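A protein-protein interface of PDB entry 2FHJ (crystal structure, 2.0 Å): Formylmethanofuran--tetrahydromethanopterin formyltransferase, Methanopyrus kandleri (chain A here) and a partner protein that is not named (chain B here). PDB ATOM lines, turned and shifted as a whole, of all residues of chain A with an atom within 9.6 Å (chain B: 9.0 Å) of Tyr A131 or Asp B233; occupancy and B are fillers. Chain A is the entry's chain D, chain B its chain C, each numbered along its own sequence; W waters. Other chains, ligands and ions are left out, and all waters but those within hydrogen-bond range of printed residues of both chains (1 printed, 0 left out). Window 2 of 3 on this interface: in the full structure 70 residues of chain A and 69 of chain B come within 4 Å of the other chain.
The backbone NH of Lys B214 lies within hydrogen-bond range of the side-chain carboxylate of Asp A129, 3.2 Å away.
NZ of Lys B210 lies within salt-bridge range of OD2 of Asp A129.
N of Gln B215 sits at hydrogen-bond distance from OD1 of Asp A129, 3.0 Å away.
The side-chain sulfur of Cys B228 sits close to the backbone carbonyl oxygen of Val A147, at 3.5 Å.
The side-chain sulfur (SG) of Cys B228 is in hydrogen-bond range of the backbone carbonyl oxygen (O) of Pro A146 (3.7 Å).
N of Thr B223 lies within hydrogen-bond range of O of Phe A127.
The side-chain hydroxyl (OH) of Tyr B216 lies within hydrogen-bond range of the side-chain amide nitrogen (NE2) of Gln A132, at 3.0 Å.
The side-chain hydroxyl (OG1) of Thr B223 is in hydrogen-bond range of the backbone carbonyl oxygen (O) of Pro A146 (2.9 Å).
The side-chain hydroxyl of Tyr A131 is in hydrogen-bond range of the side-chain carboxylate of Asp B233, 3.1 Å away.
The side-chain sulfur (SG) of Cys B228 sits at hydrogen-bond distance from the side-chain hydroxyl (OG1) of Thr B223, at 3.6 Å.
N of Lys B210 lies within hydrogen-bond range of O of Ser B222.
The backbone NH (N) of Gly A130 sits at hydrogen-bond distance from the side-chain amide oxygen (OE1) of Gln A132, 2.9 Å away.
O of Val B231 lies close to OD1 of Asn B234, 3.2 Å away.
OD1 of Asp B225 lies within salt-bridge range of NZ of Lys B210, 2.8 Å away.
The side-chain amide oxygen (OD1) of Asn B234 lies close to the backbone carbonyl oxygen (O) of Cys B228 (3.2 Å).
Tyr B216 touches Phe A126 (CE1 to O, 3.2 Å).
Phe A127 touches Ser B222.
Asp A129 touches Tyr B216.
Ser B222 touches Asp A129.
Gly A130 touches Tyr B216 (N to OH, 3.7 Å).
CG1 of Val B231 touches CE2 of Tyr A131 (3.5 Å).
Thr B230 touches Pro A146 (OG1 to CB, 3.7 Å).
Val B231 touches Pro A146.
O of Val A147 touches CD of Pro B229 (3.6 Å).
Gly A150 touches Thr B230.
Of chain B, only Tyr B216 comes within 4 Å of Gly A130.
Printed residues of chain B within 4 Å of Tyr A131: Asp B225 (3.9 Å), Val B231 (3.5 Å) and Asp B233 (3.1 Å).
Trp A143 touches none of the printed residues of chain B.
Of the printed residues of chain B, Pro A146 touches Thr B223 (2.9 Å), Cys B228 (3.7 Å), Thr B230 (3.7 Å) and Val B231 (3.8 Å).
Of the printed residues of chain A, Gln B215 touches Asp A129.
Of the printed residues of chain A, Thr B223 touches Phe A127, Gly A128, Pro A146 and Val A147.
Ala B226 touches none of the printed residues of chain A.
No residue of chain A comes within 4 Å of Glu B232.
Asp B233 touches one residue of chain A.
No residue of chain A comes within 4 Å of Asn B234.
The nearest residue of chain B that does not touch Tyr A131 is Lys B214 (4.3 Å).
The nearest residue of chain A that does not touch Asp B233 is Asp A129 (8.4 Å).
The nearest printed residue of chain B that does not touch Gly A128 is Tyr B216 (5.4 Å).
Printed residues of chain A that touch a printed residue of chain B: Phe A126, Phe A127, Gly A128, Asp A129, Gly A130, Tyr A131, Gln A132, Pro A146, Val A147 and Gly A150.
Printed residues of chain B that touch a printed residue of chain A: Lys B210, Lys B214, Gln B215, Tyr B216, Ser B222, Thr B223, Asp B225, Cys B228, Pro B229, Thr B230, Val B231 and Asp B233.
Among the printed residues, 22 pairs touch across the chains.
Among the printed residues, Asp or Glu carboxylates within 4 Å of a Lys or Arg side-chain nitrogen of the other chain: Asp A129 with Lys B210 (2.8 Å).
Water W1 lies within hydrogen-bond range of the backbone carbonyl oxygen of Gly A150 (2.6 Å), the side-chain hydroxyl of Thr B230 (2.6 Å) and the backbone carbonyl oxygen of Val A147 (3.0 Å).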
ATOM      1  N   SER A 125      10.436  -1.104  23.107  1.00  0.00           N
ATOM      2  CA  SER A 125       9.099  -1.340  23.676  1.00  0.00           C
ATOM      3  C   SER A 125       7.990  -0.469  23.046  1.00  0.00           C
ATOM      4  O   SER A 125       6.851  -0.891  22.977  1.00  0.00           O
ATOM      5  CB  SER A 125       9.133  -1.169  25.199  1.00  0.00           C
ATOM      6  OG  SER A 125       9.220   0.207  25.532  1.00  0.00           O
ATOM      7  N   PHE A 126       8.339   0.728  22.567  1.00  0.00           N
ATOM      8  CA  PHE A 126       7.368   1.614  21.908  1.00  0.00           C
ATOM      9  C   PHE A 126       6.730   1.016  20.638  1.00  0.00           C
ATOM     10  O   PHE A 126       5.688   1.484  20.178  1.00  0.00           O
ATOM     11  CB  PHE A 126       8.005   2.967  21.579  1.00  0.00           C
ATOM     12  CG  PHE A 126       8.319   3.792  22.793  1.00  0.00           C
ATOM     13  CD1 PHE A 126       9.538   3.663  23.448  1.00  0.00           C
ATOM     14  CD2 PHE A 126       7.396   4.691  23.293  1.00  0.00           C
ATOM     15  CE1 PHE A 126       9.819   4.423  24.578  1.00  0.00           C
ATOM     16  CE2 PHE A 126       7.668   5.440  24.406  1.00  0.00           C
ATOM     17  CZ  PHE A 126       8.879   5.306  25.051  1.00  0.00           C
ATOM     18  N   PHE A 127       7.362  -0.010  20.082  1.00  0.00           N
ATOM     19  CA  PHE A 127       6.757  -0.858  19.054  1.00  0.00           C
ATOM     20  C   PHE A 127       5.415  -1.480  19.493  1.00  0.00           C
ATOM     21  O   PHE A 127       4.549  -1.708  18.644  1.00  0.00           O
ATOM     22  CB  PHE A 127       7.754  -1.965  18.666  1.00  0.00           C
ATOM     23  CG  PHE A 127       7.365  -2.765  17.446  1.00  0.00           C
ATOM     24  CD1 PHE A 127       6.862  -4.054  17.570  1.00  0.00           C
ATOM     25  CD2 PHE A 127       7.520  -2.242  16.178  1.00  0.00           C
ATOM     26  CE1 PHE A 127       6.508  -4.816  16.446  1.00  0.00           C
ATOM     27  CE2 PHE A 127       7.169  -2.985  15.050  1.00  0.00           C
ATOM     28  CZ  PHE A 127       6.668  -4.295  15.196  1.00  0.00           C
ATOM     29  N   GLY A 128       5.253  -1.744  20.798  1.00  0.00           N
ATOM     30  CA  GLY A 128       4.024  -2.325  21.371  1.00  0.00           C
ATOM     31  C   GLY A 128       2.783  -1.431  21.321  1.00  0.00           C
ATOM     32  O   GLY A 128       1.666  -1.895  21.571  1.00  0.00           O
ATOM     33  N   ASP A 129       2.989  -0.150  21.022  1.00  0.00           N
ATOM     34  CA  ASP A 129       1.899   0.820  20.782  1.00  0.00           C
ATOM     35  C   ASP A 129       0.923   0.966  21.954  1.00  0.00           C
ATOM     36  O   ASP A 129      -0.295   1.045  21.742  1.00  0.00           O
ATOM     37  CB  ASP A 129       1.146   0.441  19.499  1.00  0.00           C
ATOM     38  CG  ASP A 129       0.514   1.650  18.782  1.00  0.00           C
ATOM     39  OD1 ASP A 129       0.721   2.826  19.200  1.00  0.00           O
ATOM     40  OD2 ASP A 129      -0.179   1.423  17.755  1.00  0.00           O
ATOM     41  N   GLY A 130       1.464   1.008  23.175  1.00  0.00           N
ATOM     42  CA  GLY A 130       0.670   1.139  24.386  1.00  0.00           C
ATOM     43  C   GLY A 130       0.486  -0.174  25.104  1.00  0.00           C
ATOM     44  O   GLY A 130       0.301  -0.175  26.319  1.00  0.00           O
ATOM     45  N   TYR A 131       0.546  -1.295  24.379  1.00  0.00           N
ATOM     46  CA  TYR A 131       0.336  -2.613  25.006  1.00  0.00           C
ATOM     47  C   TYR A 131       1.593  -3.247  25.630  1.00  0.00           C
ATOM     48  O   TYR A 131       1.515  -4.339  26.195  1.00  0.00           O
ATOM     49  CB  TYR A 131      -0.266  -3.585  23.993  1.00  0.00           C
ATOM     50  CG  TYR A 131      -1.557  -3.104  23.369  1.00  0.00           C
ATOM     51  CD1 TYR A 131      -1.551  -2.439  22.142  1.00  0.00           C
ATOM     52  CD2 TYR A 131      -2.790  -3.325  24.000  1.00  0.00           C
ATOM     53  CE1 TYR A 131      -2.736  -1.996  21.554  1.00  0.00           C
ATOM     54  CE2 TYR A 131      -3.984  -2.888  23.421  1.00  0.00           C
ATOM     55  CZ  TYR A 131      -3.946  -2.222  22.194  1.00  0.00           C
ATOM     56  OH  TYR A 131      -5.103  -1.777  21.596  1.00  0.00           O
ATOM     57  N   GLN A 132       2.749  -2.593  25.517  1.00  0.00           N
ATOM     58  CA  GLN A 132       3.971  -3.124  26.125  1.00  0.00           C
ATOM     59  C   GLN A 132       3.894  -3.059  27.627  1.00  0.00           C
ATOM     60  O   GLN A 132       3.217  -2.201  28.182  1.00  0.00           O
ATOM     61  CB  GLN A 132       5.228  -2.386  25.657  1.00  0.00           C
ATOM     62  CG  GLN A 132       5.288  -0.872  26.008  1.00  0.00           C
ATOM     63  CD  GLN A 132       4.672   0.004  24.928  1.00  0.00           C
ATOM     64  OE1 GLN A 132       3.828  -0.454  24.161  1.00  0.00           O
ATOM     65  NE2 GLN A 132       5.089   1.266  24.859  1.00  0.00           N
ATOM     66  N   GLU A 133       4.635  -3.944  28.270  1.00  0.00           N
ATOM     67  CA  GLU A 133       4.543  -4.127  29.690  1.00  0.00           C
ATOM     68  C   GLU A 133       5.931  -4.404  30.259  1.00  0.00           C
ATOM     69  O   GLU A 133       6.615  -5.331  29.813  1.00  0.00           O
ATOM     70  CB  GLU A 133       3.606  -5.284  29.988  1.00  0.00           C
ATOM     71  N   GLU A 134       6.336  -3.600  31.242  1.00  0.00           N
ATOM     72  CA  GLU A 134       7.569  -3.838  31.977  1.00  0.00           C
ATOM     73  C   GLU A 134       7.322  -5.012  32.923  1.00  0.00           C
ATOM     74  O   GLU A 134       6.193  -5.200  33.386  1.00  0.00           O
ATOM     75  CB  GLU A 134       7.988  -2.584  32.740  1.00  0.00           C
ATOM     76  CG  GLU A 134       9.344  -2.699  33.412  1.00  0.00           C
ATOM     77  N   TRP A 143      11.118  -5.859  28.997  1.00  0.00           N
ATOM     78  CA  TRP A 143       9.883  -5.413  28.374  1.00  0.00           C
ATOM     79  C   TRP A 143       9.236  -6.543  27.579  1.00  0.00           C
ATOM     80  O   TRP A 143       9.881  -7.159  26.722  1.00  0.00           O
ATOM     81  CB  TRP A 143      10.145  -4.239  27.446  1.00  0.00           C
ATOM     82  CG  TRP A 143      10.411  -2.994  28.179  1.00  0.00           C
ATOM     83  CD1 TRP A 143      11.625  -2.533  28.597  1.00  0.00           C
ATOM     84  CD2 TRP A 143       9.439  -2.033  28.621  1.00  0.00           C
ATOM     85  NE1 TRP A 143      11.471  -1.343  29.263  1.00  0.00           N
ATOM     86  CE2 TRP A 143      10.140  -1.014  29.296  1.00  0.00           C
ATOM     87  CE3 TRP A 143       8.048  -1.938  28.512  1.00  0.00           C
ATOM     88  CZ2 TRP A 143       9.499   0.095  29.848  1.00  0.00           C
ATOM     89  CZ3 TRP A 143       7.414  -0.837  29.064  1.00  0.00           C
ATOM     90  CH2 TRP A 143       8.139   0.162  29.724  1.00  0.00           C
ATOM     91  N   LYS A 144       7.963  -6.808  27.883  1.00  0.00           N
ATOM     92  CA  LYS A 144       7.152  -7.789  27.165  1.00  0.00           C
ATOM     93  C   LYS A 144       6.367  -7.054  26.077  1.00  0.00           C
ATOM     94  O   LYS A 144       5.373  -6.389  26.348  1.00  0.00           O
ATOM     95  CB  LYS A 144       6.230  -8.533  28.134  1.00  0.00           C
ATOM     96  CG  LYS A 144       6.970  -9.125  29.326  1.00  0.00           C
ATOM     97  CD  LYS A 144       6.257 -10.334  29.954  1.00  0.00           C
ATOM     98  CE  LYS A 144       4.989  -9.929  30.664  1.00  0.00           C
ATOM     99  NZ  LYS A 144       4.322 -11.067  31.379  1.00  0.00           N
ATOM    100  N   ILE A 145       6.854  -7.151  24.846  1.00  0.00           N
ATOM    101  CA  ILE A 145       6.295  -6.429  23.715  1.00  0.00           C
ATOM    102  C   ILE A 145       5.361  -7.331  22.918  1.00  0.00           C
ATOM    103  O   ILE A 145       5.801  -8.359  22.399  1.00  0.00           O
ATOM    104  CB  ILE A 145       7.397  -5.950  22.777  1.00  0.00           C
ATOM    105  CG1 ILE A 145       8.406  -5.084  23.541  1.00  0.00           C
ATOM    106  CG2 ILE A 145       6.786  -5.208  21.602  1.00  0.00           C
ATOM    107  CD1 ILE A 145       9.588  -4.627  22.710  1.00  0.00           C
ATOM    108  N   PRO A 146       4.067  -6.960  22.814  1.00  0.00           N
ATOM    109  CA  PRO A 146       3.166  -7.847  22.089  1.00  0.00           C
ATOM    110  C   PRO A 146       3.467  -7.841  20.602  1.00  0.00           C
ATOM    111  O   PRO A 146       3.619  -6.780  19.985  1.00  0.00           O
ATOM    112  CB  PRO A 146       1.770  -7.284  22.368  1.00  0.00           C
ATOM    113  CG  PRO A 146       1.950  -6.046  23.124  1.00  0.00           C
ATOM    114  CD  PRO A 146       3.386  -5.763  23.337  1.00  0.00           C
ATOM    115  N   VAL A 147       3.568  -9.037  20.045  1.00  0.00           N
ATOM    116  CA  VAL A 147       3.892  -9.212  18.645  1.00  0.00           C
ATOM    117  C   VAL A 147       2.942 -10.251  18.135  1.00  0.00           C
ATOM    118  O   VAL A 147       2.289 -10.906  18.940  1.00  0.00           O
ATOM    119  CB  VAL A 147       5.368  -9.644  18.440  1.00  0.00           C
ATOM    120  CG1 VAL A 147       6.288  -8.494  18.796  1.00  0.00           C
ATOM    121  CG2 VAL A 147       5.730 -10.899  19.252  1.00  0.00           C
ATOM    122  N   GLY A 150       3.202 -13.643  19.606  1.00  0.00           N
ATOM    123  CA  GLY A 150       2.992 -13.763  21.041  1.00  0.00           C
ATOM    124  C   GLY A 150       3.634 -12.574  21.729  1.00  0.00           C
ATOM    125  O   GLY A 150       3.077 -11.470  21.723  1.00  0.00           O
ATOM    126  N   GLU A 151       4.821 -12.775  22.294  1.00  0.00           N
ATOM    127  CA  GLU A 151       5.554 -11.663  22.911  1.00  0.00           C
ATOM    128  C   GLU A 151       6.997 -11.656  22.481  1.00  0.00           C
ATOM    129  O   GLU A 151       7.544 -12.701  22.181  1.00  0.00           O
ATOM    130  CB  GLU A 151       5.480 -11.751  24.431  1.00  0.00           C
ATOM    131  CG  GLU A 151       4.181 -11.216  24.982  1.00  0.00           C
ATOM    132  CD  GLU A 151       4.003 -11.486  26.461  1.00  0.00           C
ATOM    133  OE1 GLU A 151       4.696 -12.384  26.993  1.00  0.00           O
ATOM    134  OE2 GLU A 151       3.159 -10.802  27.086  1.00  0.00           O
ATOM    135  N   PHE A 152       7.582 -10.462  22.414  1.00  0.00           N
ATOM    136  CA  PHE A 152       9.028 -10.298  22.329  1.00  0.00           C
ATOM    137  C   PHE A 152       9.557  -9.833  23.670  1.00  0.00           C
ATOM    138  O   PHE A 152       9.226  -8.745  24.126  1.00  0.00           O
ATOM    139  CB  PHE A 152       9.431  -9.270  21.267  1.00  0.00           C
ATOM    140  CG  PHE A 152      10.921  -9.031  21.181  1.00  0.00           C
ATOM    141  CD1 PHE A 152      11.813 -10.098  21.142  1.00  0.00           C
ATOM    142  CD2 PHE A 152      11.435  -7.742  21.116  1.00  0.00           C
ATOM    143  CE1 PHE A 152      13.173  -9.887  21.073  1.00  0.00           C
ATOM    144  CE2 PHE A 152      12.796  -7.528  21.021  1.00  0.00           C
ATOM    145  CZ  PHE A 152      13.663  -8.595  21.000  1.00  0.00           C
ATOM    146  N   LYS B 210       2.679  -2.590  11.129  1.00  0.00           N
ATOM    147  CA  LYS B 210       1.746  -1.770  10.395  1.00  0.00           C
ATOM    148  C   LYS B 210       2.369  -0.379  10.140  1.00  0.00           C
ATOM    149  O   LYS B 210       3.336   0.020  10.790  1.00  0.00           O
ATOM    150  CB  LYS B 210       0.448  -1.645  11.193  1.00  0.00           C
ATOM    151  CG  LYS B 210       0.490  -0.644  12.374  1.00  0.00           C
ATOM    152  CD  LYS B 210      -0.722  -0.822  13.312  1.00  0.00           C
ATOM    153  CE  LYS B 210      -0.678   0.109  14.533  1.00  0.00           C
ATOM    154  NZ  LYS B 210       0.168  -0.419  15.669  1.00  0.00           N
ATOM    155  N   LYS B 214      -0.269   4.352  16.531  1.00  0.00           N
ATOM    156  CA  LYS B 214      -1.367   5.054  17.204  1.00  0.00           C
ATOM    157  C   LYS B 214      -0.878   6.103  18.209  1.00  0.00           C
ATOM    158  O   LYS B 214      -1.400   7.222  18.230  1.00  0.00           O
ATOM    159  CB  LYS B 214      -2.312   4.071  17.909  1.00  0.00           C
ATOM    160  CG  LYS B 214      -3.466   3.611  17.034  1.00  0.00           C
ATOM    161  CD  LYS B 214      -4.328   2.550  17.720  1.00  0.00           C
ATOM    162  CE  LYS B 214      -3.749   1.146  17.594  1.00  0.00           C
ATOM    163  NZ  LYS B 214      -4.824   0.124  17.768  1.00  0.00           N
ATOM    164  N   GLN B 215       0.114   5.752  19.031  1.00  0.00           N
ATOM    165  CA  GLN B 215       0.537   6.626  20.146  1.00  0.00           C
ATOM    166  C   GLN B 215       1.750   7.534  19.866  1.00  0.00           C
ATOM    167  O   GLN B 215       1.880   8.578  20.493  1.00  0.00           O
ATOM    168  CB  GLN B 215       0.844   5.795  21.392  1.00  0.00           C
ATOM    169  CG  GLN B 215      -0.147   4.710  21.730  1.00  0.00           C
ATOM    170  CD  GLN B 215      -1.572   5.188  21.871  1.00  0.00           C
ATOM    171  OE1 GLN B 215      -2.512   4.407  21.707  1.00  0.00           O
ATOM    172  NE2 GLN B 215      -1.751   6.464  22.182  1.00  0.00           N
ATOM    173  N   TYR B 216       2.614   7.137  18.923  1.00  0.00           N
ATOM    174  CA  TYR B 216       3.989   7.672  18.810  1.00  0.00           C
ATOM    175  C   TYR B 216       4.308   8.243  17.418  1.00  0.00           C
ATOM    176  O   TYR B 216       4.380   7.506  16.441  1.00  0.00           O
ATOM    177  CB  TYR B 216       5.006   6.575  19.190  1.00  0.00           C
ATOM    178  CG  TYR B 216       4.666   5.832  20.488  1.00  0.00           C
ATOM    179  CD1 TYR B 216       4.460   4.450  20.501  1.00  0.00           C
ATOM    180  CD2 TYR B 216       4.529   6.518  21.697  1.00  0.00           C
ATOM    181  CE1 TYR B 216       4.131   3.782  21.680  1.00  0.00           C
ATOM    182  CE2 TYR B 216       4.201   5.852  22.870  1.00  0.00           C
ATOM    183  CZ  TYR B 216       4.005   4.487  22.852  1.00  0.00           C
ATOM    184  OH  TYR B 216       3.692   3.832  24.016  1.00  0.00           O
ATOM    185  N   SER B 222       5.046   0.052  13.483  1.00  0.00           N
ATOM    186  CA  SER B 222       4.814  -0.428  14.843  1.00  0.00           C
ATOM    187  C   SER B 222       4.064  -1.746  14.778  1.00  0.00           C
ATOM    188  O   SER B 222       3.793  -2.262  13.689  1.00  0.00           O
ATOM    189  CB  SER B 222       4.084   0.629  15.687  1.00  0.00           C
ATOM    190  OG  SER B 222       2.788   0.886  15.194  1.00  0.00           O
ATOM    191  N   THR B 223       3.765  -2.323  15.930  1.00  0.00           N
ATOM    192  CA  THR B 223       3.234  -3.674  15.957  1.00  0.00           C
ATOM    193  C   THR B 223       1.866  -3.735  15.273  1.00  0.00           C
ATOM    194  O   THR B 223       1.083  -2.787  15.360  1.00  0.00           O
ATOM    195  CB  THR B 223       3.160  -4.219  17.402  1.00  0.00           C
ATOM    196  OG1 THR B 223       3.056  -5.651  17.373  1.00  0.00           O
ATOM    197  CG2 THR B 223       1.995  -3.605  18.182  1.00  0.00           C
ATOM    198  N   ASN B 224       1.597  -4.834  14.566  1.00  0.00           N
ATOM    199  CA  ASN B 224       0.248  -5.127  14.068  1.00  0.00           C
ATOM    200  C   ASN B 224      -0.621  -5.685  15.205  1.00  0.00           C
ATOM    201  O   ASN B 224      -0.865  -6.896  15.279  1.00  0.00           O
ATOM    202  CB  ASN B 224       0.309  -6.123  12.901  1.00  0.00           C
ATOM    203  CG  ASN B 224      -1.031  -6.304  12.200  1.00  0.00           C
ATOM    204  OD1 ASN B 224      -1.978  -5.549  12.423  1.00  0.00           O
ATOM    205  ND2 ASN B 224      -1.109  -7.318  11.344  1.00  0.00           N
ATOM    206  N   ASP B 225      -1.080  -4.801  16.090  1.00  0.00           N
ATOM    207  CA  ASP B 225      -1.822  -5.205  17.311  1.00  0.00           C
ATOM    208  C   ASP B 225      -3.113  -6.006  17.076  1.00  0.00           C
ATOM    209  O   ASP B 225      -3.541  -6.782  17.932  1.00  0.00           O
ATOM    210  CB  ASP B 225      -2.102  -3.993  18.227  1.00  0.00           C
ATOM    211  CG  ASP B 225      -2.547  -2.758  17.465  1.00  0.00           C
ATOM    212  OD1 ASP B 225      -1.761  -2.229  16.645  1.00  0.00           O
ATOM    213  OD2 ASP B 225      -3.687  -2.306  17.697  1.00  0.00           O
ATOM    214  N   ALA B 226      -3.736  -5.808  15.925  1.00  0.00           N
ATOM    215  CA  ALA B 226      -4.921  -6.555  15.523  1.00  0.00           C
ATOM    216  C   ALA B 226      -4.672  -8.068  15.464  1.00  0.00           C
ATOM    217  O   ALA B 226      -5.593  -8.830  15.709  1.00  0.00           O
ATOM    218  CB  ALA B 226      -5.406  -6.050  14.191  1.00  0.00           C
ATOM    219  N   TYR B 227      -3.444  -8.489  15.155  1.00  0.00           N
ATOM    220  CA  TYR B 227      -3.089  -9.920  15.128  1.00  0.00           C
ATOM    221  C   TYR B 227      -2.182 -10.355  16.285  1.00  0.00           C
ATOM    222  O   TYR B 227      -1.553 -11.403  16.214  1.00  0.00           O
ATOM    223  CB  TYR B 227      -2.407 -10.271  13.809  1.00  0.00           C
ATOM    224  CG  TYR B 227      -3.285 -10.302  12.573  1.00  0.00           C
ATOM    225  CD1 TYR B 227      -4.680 -10.341  12.647  1.00  0.00           C
ATOM    226  CD2 TYR B 227      -2.706 -10.357  11.319  1.00  0.00           C
ATOM    227  CE1 TYR B 227      -5.462 -10.387  11.504  1.00  0.00           C
ATOM    228  CE2 TYR B 227      -3.480 -10.403  10.172  1.00  0.00           C
ATOM    229  CZ  TYR B 227      -4.858 -10.418  10.268  1.00  0.00           C
ATOM    230  OH  TYR B 227      -5.607 -10.474   9.107  1.00  0.00           O
ATOM    231  N   CYS B 228      -2.129  -9.571  17.356  1.00  0.00           N
ATOM    232  CA  CYS B 228      -1.386  -9.966  18.553  1.00  0.00           C
ATOM    233  C   CYS B 228      -2.252 -10.814  19.506  1.00  0.00           C
ATOM    234  O   CYS B 228      -3.227 -10.306  20.053  1.00  0.00           O
ATOM    235  CB  CYS B 228      -0.885  -8.711  19.257  1.00  0.00           C
ATOM    236  SG  CYS B 228       0.493  -7.924  18.341  1.00  0.00           S
ATOM    237  N   PRO B 229      -1.895 -12.098  19.724  1.00  0.00           N
ATOM    238  CA  PRO B 229      -2.748 -12.928  20.576  1.00  0.00           C
ATOM    239  C   PRO B 229      -2.905 -12.405  22.011  1.00  0.00           C
ATOM    240  O   PRO B 229      -3.949 -12.632  22.624  1.00  0.00           O
ATOM    241  CB  PRO B 229      -2.062 -14.308  20.553  1.00  0.00           C
ATOM    242  CG  PRO B 229      -1.191 -14.285  19.388  1.00  0.00           C
ATOM    243  CD  PRO B 229      -0.737 -12.858  19.233  1.00  0.00           C
ATOM    244  N   THR B 230      -1.894 -11.721  22.544  1.00  0.00           N
ATOM    245  CA  THR B 230      -1.945 -11.255  23.926  1.00  0.00           C
ATOM    246  C   THR B 230      -2.585  -9.857  24.062  1.00  0.00           C
ATOM    247  O   THR B 230      -2.787  -9.397  25.186  1.00  0.00           O
ATOM    248  CB  THR B 230      -0.549 -11.233  24.593  1.00  0.00           C
ATOM    249  OG1 THR B 230       0.245 -10.222  23.979  1.00  0.00           O
ATOM    250  CG2 THR B 230       0.152 -12.615  24.504  1.00  0.00           C
ATOM    251  N   VAL B 231      -2.884  -9.187  22.939  1.00  0.00           N
ATOM    252  CA  VAL B 231      -3.603  -7.885  22.939  1.00  0.00           C
ATOM    253  C   VAL B 231      -5.109  -8.139  23.077  1.00  0.00           C
ATOM    254  O   VAL B 231      -5.697  -8.868  22.262  1.00  0.00           O
ATOM    255  CB  VAL B 231      -3.337  -7.062  21.640  1.00  0.00           C
ATOM    256  CG1 VAL B 231      -4.223  -5.827  21.558  1.00  0.00           C
ATOM    257  CG2 VAL B 231      -1.888  -6.636  21.559  1.00  0.00           C
ATOM    258  N   GLU B 232      -5.725  -7.539  24.100  1.00  0.00           N
ATOM    259  CA  GLU B 232      -7.119  -7.827  24.497  1.00  0.00           C
ATOM    260  C   GLU B 232      -8.190  -7.620  23.413  1.00  0.00           C
ATOM    261  O   GLU B 232      -9.164  -8.370  23.336  1.00  0.00           O
ATOM    262  N   ASP B 233      -7.987  -6.613  22.571  1.00  0.00           N
ATOM    263  CA  ASP B 233      -8.966  -6.224  21.553  1.00  0.00           C
ATOM    264  C   ASP B 233      -8.603  -6.726  20.149  1.00  0.00           C
ATOM    265  O   ASP B 233      -8.950  -6.088  19.157  1.00  0.00           O
ATOM    266  CB  ASP B 233      -9.077  -4.688  21.532  1.00  0.00           C
ATOM    267  CG  ASP B 233      -7.704  -4.002  21.532  1.00  0.00           C
ATOM    268  OD1 ASP B 233      -7.173  -3.712  20.431  1.00  0.00           O
ATOM    269  OD2 ASP B 233      -7.148  -3.789  22.640  1.00  0.00           O
ATOM    270  N   ASN B 234      -7.936  -7.874  20.048  1.00  0.00           N
ATOM    271  CA  ASN B 234      -7.414  -8.327  18.753  1.00  0.00           C
ATOM    272  C   ASN B 234      -8.510  -8.769  17.775  1.00  0.00           C
ATOM    273  O   ASN B 234      -9.643  -9.003  18.171  1.00  0.00           O
ATOM    274  CB  ASN B 234      -6.353  -9.419  18.939  1.00  0.00           C
ATOM    275  CG  ASN B 234      -6.908 -10.710  19.512  1.00  0.00           C
ATOM    276  OD1 ASN B 234      -6.236 -11.385  20.292  1.00  0.00           O
ATOM    277  ND2 ASN B 234      -8.120 -11.069  19.123  1.00  0.00           N
ATOM    278  N   GLU B 235      -8.152  -8.871  16.500  1.00  0.00           N
ATOM    279  CA  GLU B 235      -9.065  -9.313  15.455  1.00  0.00           C
ATOM    280  C   GLU B 235      -8.759 -10.739  15.015  1.00  0.00           C
ATOM    281  O   GLU B 235      -8.855 -11.069  13.833  1.00  0.00           O
ATOM    282  CB  GLU B 235      -8.970  -8.366  14.264  1.00  0.00           C
ATOM    283  CG  GLU B 235      -9.308  -6.927  14.654  1.00  0.00           C
ATOM    284  CD  GLU B 235      -9.472  -6.005  13.465  1.00  0.00           C
ATOM    285  OE1 GLU B 235      -9.073  -6.398  12.345  1.00  0.00           O
ATOM    286  OE2 GLU B 235      -9.991  -4.876  13.666  1.00  0.00           O
ATOM    287  N   LEU B 236      -8.418 -11.587  15.979  1.00  0.00           N
ATOM    288  CA  LEU B 236      -8.040 -12.958  15.690  1.00  0.00           C
ATOM    289  C   LEU B 236      -9.181 -13.905  16.003  1.00  0.00           C
ATOM    290  O   LEU B 236      -9.872 -13.740  17.002  1.00  0.00           O
ATOM    291  CB  LEU B 236      -6.841 -13.361  16.537  1.00  0.00           C
ATOM    292  CG  LEU B 236      -5.513 -12.691  16.219  1.00  0.00           C
ATOM    293  CD1 LEU B 236      -4.503 -13.068  17.271  1.00  0.00           C
ATOM    294  CD2 LEU B 236      -5.021 -13.063  14.823  1.00  0.00           C
HETATM  295  O   HOH W   1       0.744 -10.340  21.407  1.00  0.00           O
